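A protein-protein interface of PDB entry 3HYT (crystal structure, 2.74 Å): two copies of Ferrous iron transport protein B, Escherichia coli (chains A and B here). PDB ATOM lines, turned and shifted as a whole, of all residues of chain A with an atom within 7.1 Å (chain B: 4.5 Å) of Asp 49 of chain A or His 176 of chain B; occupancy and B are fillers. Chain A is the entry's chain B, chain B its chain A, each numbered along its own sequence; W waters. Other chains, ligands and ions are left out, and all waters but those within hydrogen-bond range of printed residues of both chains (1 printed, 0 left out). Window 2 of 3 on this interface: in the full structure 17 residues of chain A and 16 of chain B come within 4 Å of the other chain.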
ATOM      1  N   LYS A   2      16.031   7.060 -20.365  1.00  0.00           N
ATOM      2  CA  LYS A   2      14.978   8.027 -19.944  1.00  0.00           C
ATOM      3  C   LYS A   2      14.058   8.323 -21.126  1.00  0.00           C
ATOM      4  O   LYS A   2      14.526   8.640 -22.219  1.00  0.00           O
ATOM      5  CB  LYS A   2      15.616   9.322 -19.428  1.00  0.00           C
ATOM      6  CG  LYS A   2      14.887   9.987 -18.251  1.00  0.00           C
ATOM      7  CD  LYS A   2      13.518  10.587 -18.613  1.00  0.00           C
ATOM      8  CE  LYS A   2      13.599  11.609 -19.749  1.00  0.00           C
ATOM      9  NZ  LYS A   2      14.447  12.799 -19.434  1.00  0.00           N
ATOM     10  N   LYS A   3      12.751   8.224 -20.900  1.00  0.00           N
ATOM     11  CA  LYS A   3      11.780   8.365 -21.978  1.00  0.00           C
ATOM     12  C   LYS A   3      11.344   9.816 -22.190  1.00  0.00           C
ATOM     13  O   LYS A   3      10.882  10.478 -21.258  1.00  0.00           O
ATOM     14  CB  LYS A   3      10.569   7.459 -21.729  1.00  0.00           C
ATOM     15  N   LEU A   4      11.512  10.301 -23.420  1.00  0.00           N
ATOM     16  CA  LEU A   4      11.018  11.619 -23.828  1.00  0.00           C
ATOM     17  C   LEU A   4       9.961  11.484 -24.909  1.00  0.00           C
ATOM     18  O   LEU A   4      10.060  10.620 -25.785  1.00  0.00           O
ATOM     19  CB  LEU A   4      12.151  12.496 -24.375  1.00  0.00           C
ATOM     20  CG  LEU A   4      13.085  13.251 -23.432  1.00  0.00           C
ATOM     21  CD1 LEU A   4      14.111  14.002 -24.259  1.00  0.00           C
ATOM     22  CD2 LEU A   4      12.321  14.206 -22.523  1.00  0.00           C
ATOM     23  N   SER A  46      16.318   6.655 -30.669  1.00  0.00           N
ATOM     24  CA  SER A  46      17.120   6.916 -29.479  1.00  0.00           C
ATOM     25  C   SER A  46      18.178   7.992 -29.701  1.00  0.00           C
ATOM     26  O   SER A  46      18.630   8.230 -30.825  1.00  0.00           O
ATOM     27  CB  SER A  46      17.762   5.628 -28.960  1.00  0.00           C
ATOM     28  OG  SER A  46      18.585   5.042 -29.948  1.00  0.00           O
ATOM     29  N   THR A  47      18.543   8.646 -28.607  1.00  0.00           N
ATOM     30  CA  THR A  47      19.610   9.634 -28.586  1.00  0.00           C
ATOM     31  C   THR A  47      20.652   9.182 -27.544  1.00  0.00           C
ATOM     32  O   THR A  47      20.570   8.056 -27.050  1.00  0.00           O
ATOM     33  CB  THR A  47      19.045  11.074 -28.360  1.00  0.00           C
ATOM     34  OG1 THR A  47      20.112  11.982 -28.075  1.00  0.00           O
ATOM     35  CG2 THR A  47      18.054  11.116 -27.230  1.00  0.00           C
ATOM     36  N   THR A  48      21.636  10.021 -27.231  1.00  0.00           N
ATOM     37  CA  THR A  48      22.703   9.637 -26.296  1.00  0.00           C
ATOM     38  C   THR A  48      22.185   9.389 -24.874  1.00  0.00           C
ATOM     39  O   THR A  48      22.672   8.498 -24.177  1.00  0.00           O
ATOM     40  CB  THR A  48      23.851  10.675 -26.274  1.00  0.00           C
ATOM     41  OG1 THR A  48      24.330  10.882 -27.604  1.00  0.00           O
ATOM     42  CG2 THR A  48      25.012  10.200 -25.414  1.00  0.00           C
ATOM     43  N   ASP A  49      21.189  10.169 -24.464  1.00  0.00           N
ATOM     44  CA  ASP A  49      20.677  10.118 -23.099  1.00  0.00           C
ATOM     45  C   ASP A  49      19.246   9.601 -22.981  1.00  0.00           C
ATOM     46  O   ASP A  49      18.833   9.154 -21.909  1.00  0.00           O
ATOM     47  CB  ASP A  49      20.780  11.502 -22.451  1.00  0.00           C
ATOM     48  CG  ASP A  49      22.209  11.880 -22.097  1.00  0.00           C
ATOM     49  OD1 ASP A  49      23.072  10.976 -22.020  1.00  0.00           O
ATOM     50  OD2 ASP A  49      22.466  13.086 -21.886  1.00  0.00           O
ATOM     51  N   HIS A  50      18.493   9.658 -24.075  1.00  0.00           N
ATOM     52  CA  HIS A  50      17.061   9.383 -24.019  1.00  0.00           C
ATOM     53  C   HIS A  50      16.574   8.394 -25.070  1.00  0.00           C
ATOM     54  O   HIS A  50      17.188   8.230 -26.125  1.00  0.00           O
ATOM     55  CB  HIS A  50      16.259  10.679 -24.153  1.00  0.00           C
ATOM     56  CG  HIS A  50      16.664  11.753 -23.195  1.00  0.00           C
ATOM     57  ND1 HIS A  50      17.334  12.888 -23.593  1.00  0.00           N
ATOM     58  CD2 HIS A  50      16.490  11.867 -21.857  1.00  0.00           C
ATOM     59  CE1 HIS A  50      17.555  13.658 -22.541  1.00  0.00           C
ATOM     60  NE2 HIS A  50      17.053  13.061 -21.476  1.00  0.00           N
ATOM     61  N   GLN A  51      15.472   7.724 -24.749  1.00  0.00           N
ATOM     62  CA  GLN A  51      14.683   6.999 -25.732  1.00  0.00           C
ATOM     63  C   GLN A  51      13.478   7.885 -26.057  1.00  0.00           C
ATOM     64  O   GLN A  51      12.676   8.218 -25.179  1.00  0.00           O
ATOM     65  CB  GLN A  51      14.277   5.617 -25.202  1.00  0.00           C
ATOM     66  CG  GLN A  51      13.204   4.872 -26.018  1.00  0.00           C
ATOM     67  CD  GLN A  51      13.585   4.611 -27.480  1.00  0.00           C
ATOM     68  OE1 GLN A  51      14.762   4.511 -27.832  1.00  0.00           O
ATOM     69  NE2 GLN A  51      12.575   4.484 -28.333  1.00  0.00           N
ATOM     70  N   LYS A 160      19.673  15.987 -32.572  1.00  0.00           N
ATOM     71  CA  LYS A 160      19.855  15.034 -31.477  1.00  0.00           C
ATOM     72  C   LYS A 160      20.604  15.642 -30.292  1.00  0.00           C
ATOM     73  O   LYS A 160      20.231  15.416 -29.137  1.00  0.00           O
ATOM     74  CB  LYS A 160      20.580  13.785 -31.970  1.00  0.00           C
ATOM     75  CG  LYS A 160      19.695  12.832 -32.756  1.00  0.00           C
ATOM     76  CD  LYS A 160      20.395  11.507 -32.990  1.00  0.00           C
ATOM     77  CE  LYS A 160      19.417  10.462 -33.492  1.00  0.00           C
ATOM     78  NZ  LYS A 160      20.092   9.168 -33.811  1.00  0.00           N
ATOM     79  N   LEU A 161      21.654  16.410 -30.584  1.00  0.00           N
ATOM     80  CA  LEU A 161      22.395  17.138 -29.559  1.00  0.00           C
ATOM     81  C   LEU A 161      21.489  18.117 -28.807  1.00  0.00           C
ATOM     82  O   LEU A 161      21.508  18.172 -27.581  1.00  0.00           O
ATOM     83  CB  LEU A 161      23.589  17.873 -30.177  1.00  0.00           C
ATOM     84  CG  LEU A 161      24.595  18.532 -29.226  1.00  0.00           C
ATOM     85  CD1 LEU A 161      25.253  17.502 -28.309  1.00  0.00           C
ATOM     86  CD2 LEU A 161      25.648  19.315 -29.999  1.00  0.00           C
ATOM     87  N   ILE A 163      18.291  17.945 -28.444  1.00  0.00           N
ATOM     88  CA  ILE A 163      17.333  17.166 -27.649  1.00  0.00           C
ATOM     89  C   ILE A 163      17.923  16.754 -26.295  1.00  0.00           C
ATOM     90  O   ILE A 163      17.246  16.828 -25.272  1.00  0.00           O
ATOM     91  CB  ILE A 163      16.801  15.927 -28.430  1.00  0.00           C
ATOM     92  CG1 ILE A 163      15.865  16.369 -29.561  1.00  0.00           C
ATOM     93  CG2 ILE A 163      16.072  14.955 -27.499  1.00  0.00           C
ATOM     94  CD1 ILE A 163      15.587  15.302 -30.599  1.00  0.00           C
ATOM     95  N   ASP A 164      19.190  16.339 -26.297  1.00  0.00           N
ATOM     96  CA  ASP A 164      19.897  15.974 -25.066  1.00  0.00           C
ATOM     97  C   ASP A 164      20.209  17.175 -24.176  1.00  0.00           C
ATOM     98  O   ASP A 164      20.420  17.022 -22.969  1.00  0.00           O
ATOM     99  CB  ASP A 164      21.198  15.234 -25.387  1.00  0.00           C
ATOM    100  CG  ASP A 164      20.965  13.810 -25.864  1.00  0.00           C
ATOM    101  OD1 ASP A 164      19.849  13.273 -25.680  1.00  0.00           O
ATOM    102  OD2 ASP A 164      21.912  13.220 -26.425  1.00  0.00           O
ATOM    103  N   ARG A 165      20.250  18.363 -24.769  1.00  0.00           N
ATOM    104  CA  ARG A 165      20.577  19.571 -24.024  1.00  0.00           C
ATOM    105  C   ARG A 165      19.347  20.425 -23.760  1.00  0.00           C
ATOM    106  O   ARG A 165      19.460  21.544 -23.263  1.00  0.00           O
ATOM    107  CB  ARG A 165      21.630  20.390 -24.766  1.00  0.00           C
ATOM    108  CG  ARG A 165      23.030  19.863 -24.640  1.00  0.00           C
ATOM    109  CD  ARG A 165      23.934  20.572 -25.621  1.00  0.00           C
ATOM    110  NE  ARG A 165      25.331  20.185 -25.448  1.00  0.00           N
ATOM    111  CZ  ARG A 165      26.322  20.572 -26.245  1.00  0.00           C
ATOM    112  NH1 ARG A 165      26.072  21.363 -27.283  1.00  0.00           N
ATOM    113  NH2 ARG A 165      27.563  20.163 -26.003  1.00  0.00           N
ATOM    114  N   GLU B 173      29.934  23.578 -22.580  1.00  0.00           N
ATOM    115  CA  GLU B 173      29.976  22.147 -22.883  1.00  0.00           C
ATOM    116  C   GLU B 173      30.216  21.889 -24.376  1.00  0.00           C
ATOM    117  O   GLU B 173      29.414  22.280 -25.231  1.00  0.00           O
ATOM    118  CB  GLU B 173      28.713  21.423 -22.398  1.00  0.00           C
ATOM    119  CG  GLU B 173      28.918  19.912 -22.208  1.00  0.00           C
ATOM    120  CD  GLU B 173      27.646  19.101 -22.435  1.00  0.00           C
ATOM    121  OE1 GLU B 173      26.698  19.216 -21.623  1.00  0.00           O
ATOM    122  OE2 GLU B 173      27.603  18.340 -23.426  1.00  0.00           O
ATOM    123  N   LEU B 174      31.330  21.226 -24.672  1.00  0.00           N
ATOM    124  CA  LEU B 174      31.716  20.938 -26.049  1.00  0.00           C
ATOM    125  C   LEU B 174      31.149  19.609 -26.530  1.00  0.00           C
ATOM    126  O   LEU B 174      30.220  19.586 -27.339  1.00  0.00           O
ATOM    127  CB  LEU B 174      33.239  20.959 -26.196  1.00  0.00           C
ATOM    128  CG  LEU B 174      33.952  22.293 -25.960  1.00  0.00           C
ATOM    129  CD1 LEU B 174      35.423  22.045 -25.642  1.00  0.00           C
ATOM    130  CD2 LEU B 174      33.787  23.220 -27.163  1.00  0.00           C
ATOM    131  N   VAL B 175      31.697  18.508 -26.023  1.00  0.00           N
ATOM    132  CA  VAL B 175      31.281  17.171 -26.446  1.00  0.00           C
ATOM    133  C   VAL B 175      30.335  16.527 -25.432  1.00  0.00           C
ATOM    134  O   VAL B 175      30.637  16.451 -24.243  1.00  0.00           O
ATOM    135  CB  VAL B 175      32.491  16.237 -26.691  1.00  0.00           C
ATOM    136  CG1 VAL B 175      32.040  14.957 -27.350  1.00  0.00           C
ATOM    137  CG2 VAL B 175      33.543  16.920 -27.548  1.00  0.00           C
ATOM    138  N   HIS B 176      29.195  16.052 -25.920  1.00  0.00           N
ATOM    139  CA  HIS B 176      28.200  15.414 -25.078  1.00  0.00           C
ATOM    140  C   HIS B 176      28.389  13.897 -25.067  1.00  0.00           C
ATOM    141  O   HIS B 176      27.749  13.170 -25.831  1.00  0.00           O
ATOM    142  CB  HIS B 176      26.803  15.787 -25.561  1.00  0.00           C
ATOM    143  CG  HIS B 176      25.719  15.471 -24.582  1.00  0.00           C
ATOM    144  ND1 HIS B 176      25.360  16.332 -23.568  1.00  0.00           N
ATOM    145  CD2 HIS B 176      24.906  14.394 -24.468  1.00  0.00           C
ATOM    146  CE1 HIS B 176      24.375  15.798 -22.868  1.00  0.00           C
ATOM    147  NE2 HIS B 176      24.081  14.621 -23.393  1.00  0.00           N
ATOM    148  N   TYR B 177      29.280  13.432 -24.196  1.00  0.00           N
ATOM    149  CA  TYR B 177      29.582  12.012 -24.053  1.00  0.00           C
ATOM    150  C   TYR B 177      28.488  11.272 -23.287  1.00  0.00           C
ATOM    151  O   TYR B 177      27.792  11.861 -22.460  1.00  0.00           O
ATOM    152  CB  TYR B 177      30.899  11.827 -23.307  1.00  0.00           C
ATOM    153  CG  TYR B 177      32.111  12.402 -23.987  1.00  0.00           C
ATOM    154  CD1 TYR B 177      32.672  13.603 -23.553  1.00  0.00           C
ATOM    155  CD2 TYR B 177      32.716  11.737 -25.054  1.00  0.00           C
ATOM    156  CE1 TYR B 177      33.799  14.129 -24.166  1.00  0.00           C
ATOM    157  CE2 TYR B 177      33.843  12.255 -25.675  1.00  0.00           C
ATOM    158  CZ  TYR B 177      34.380  13.450 -25.226  1.00  0.00           C
ATOM    159  OH  TYR B 177      35.499  13.958 -25.849  1.00  0.00           O
ATOM    160  N   ALA B 178      28.348   9.976 -23.560  1.00  0.00           N
ATOM    161  CA  ALA B 178      27.460   9.119 -22.782  1.00  0.00           C
ATOM    162  C   ALA B 178      27.940   9.141 -21.337  1.00  0.00           C
ATOM    163  O   ALA B 178      29.148   9.118 -21.084  1.00  0.00           O
ATOM    164  CB  ALA B 178      27.463   7.702 -23.330  1.00  0.00           C
ATOM    165  N   ALA B 247      30.399  10.821 -30.367  1.00  0.00           N
ATOM    166  CA  ALA B 247      30.092  12.047 -29.639  1.00  0.00           C
ATOM    167  C   ALA B 247      30.916  13.209 -30.178  1.00  0.00           C
ATOM    168  O   ALA B 247      30.407  14.320 -30.358  1.00  0.00           O
ATOM    169  CB  ALA B 247      30.342  11.848 -28.153  1.00  0.00           C
HETATM  170  O   HOH W   1      25.297  11.884 -21.188  1.00  0.00           O
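The side-chain carboxylate of Glu 173 of chain B lies within salt-bridge range of the guanidinium group of Arg 165 of chain A.
O of Leu 174 of chain B is in hydrogen-bond range of NH2 of Arg 165 of chain A, at 3.0 Å.
A ring nitrogen (NE2) of His 176 of chain B lies within hydrogen-bond range of the side-chain carboxylate (OD2) of Asp 49 of chain A (2.7 Å).
The side-chain carboxylate of Glu 173 of chain B sits at hydrogen-bond distance from a ring nitrogen (ND1) of His 176 of chain B (3.0 Å).
OD1 of Asp 164 of chain A is in hydrogen-bond range of OG1 of Thr 47 of chain A (2.7 Å).
The backbone NH of Thr 48 of chain A sits close to the side-chain carboxylate of Asp 164 of chain A, 3.3 Å away.
The side-chain carboxylate (OD1) of Asp 164 of chain A is in hydrogen-bond range of a ring nitrogen (ND1) of His 50 of chain A (3.3 Å).
Among the printed residues, pairs that only touch across the chains: Thr 48 of chain A with Ala 178 of chain B (3.8 Å), Leu 161 of chain A with His 176 of chain B (3.6 Å) and Asp 164 of chain A with His 176 of chain B (3.6 Å).
Asp 49 of chain A touches one residue of chain B.
Printed residues of chain A within 4 Å of Glu 173 of chain B: Arg 165 (2.9 Å).
Printed residues of chain A within 4 Å of Leu 174 of chain B: Arg 165 (3.0 Å).
Of the printed residues of chain A, His 176 of chain B touches Asp 49 (2.7 Å), Leu 161 (3.6 Å) and Asp 164 (3.6 Å).
The nearest printed residue of chain B that does not touch Asp 49 of chain A is Tyr 177 of chain B (4.8 Å).
The nearest residue of chain A that does not touch His 176 of chain B is Thr 48 of chain A (4.1 Å).
The nearest printed residue of chain B that does not touch Leu 161 of chain A is Leu 174 of chain B (5.3 Å).
Of the 7 printed residues of chain B, 4 touch a printed residue of chain A.
Hydrophobic or aromatic side chains of chain B that line the printed part of chain A: His 176.
Along chain B the printed residues that touch a printed residue of chain A span positions 173 to 178.
Of the 14 printed residues of chain A, 5 touch a printed residue of chain B.
Printed residues of chain A that touch a printed residue of chain B: Thr 48, Asp 49, Leu 161, Asp 164 and Arg 165.
No position is printed for both chains.
Water W1 bridges the side-chain carboxylate of Asp 49 of chain A and the backbone carbonyl oxygen of Tyr 177 of chain B.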
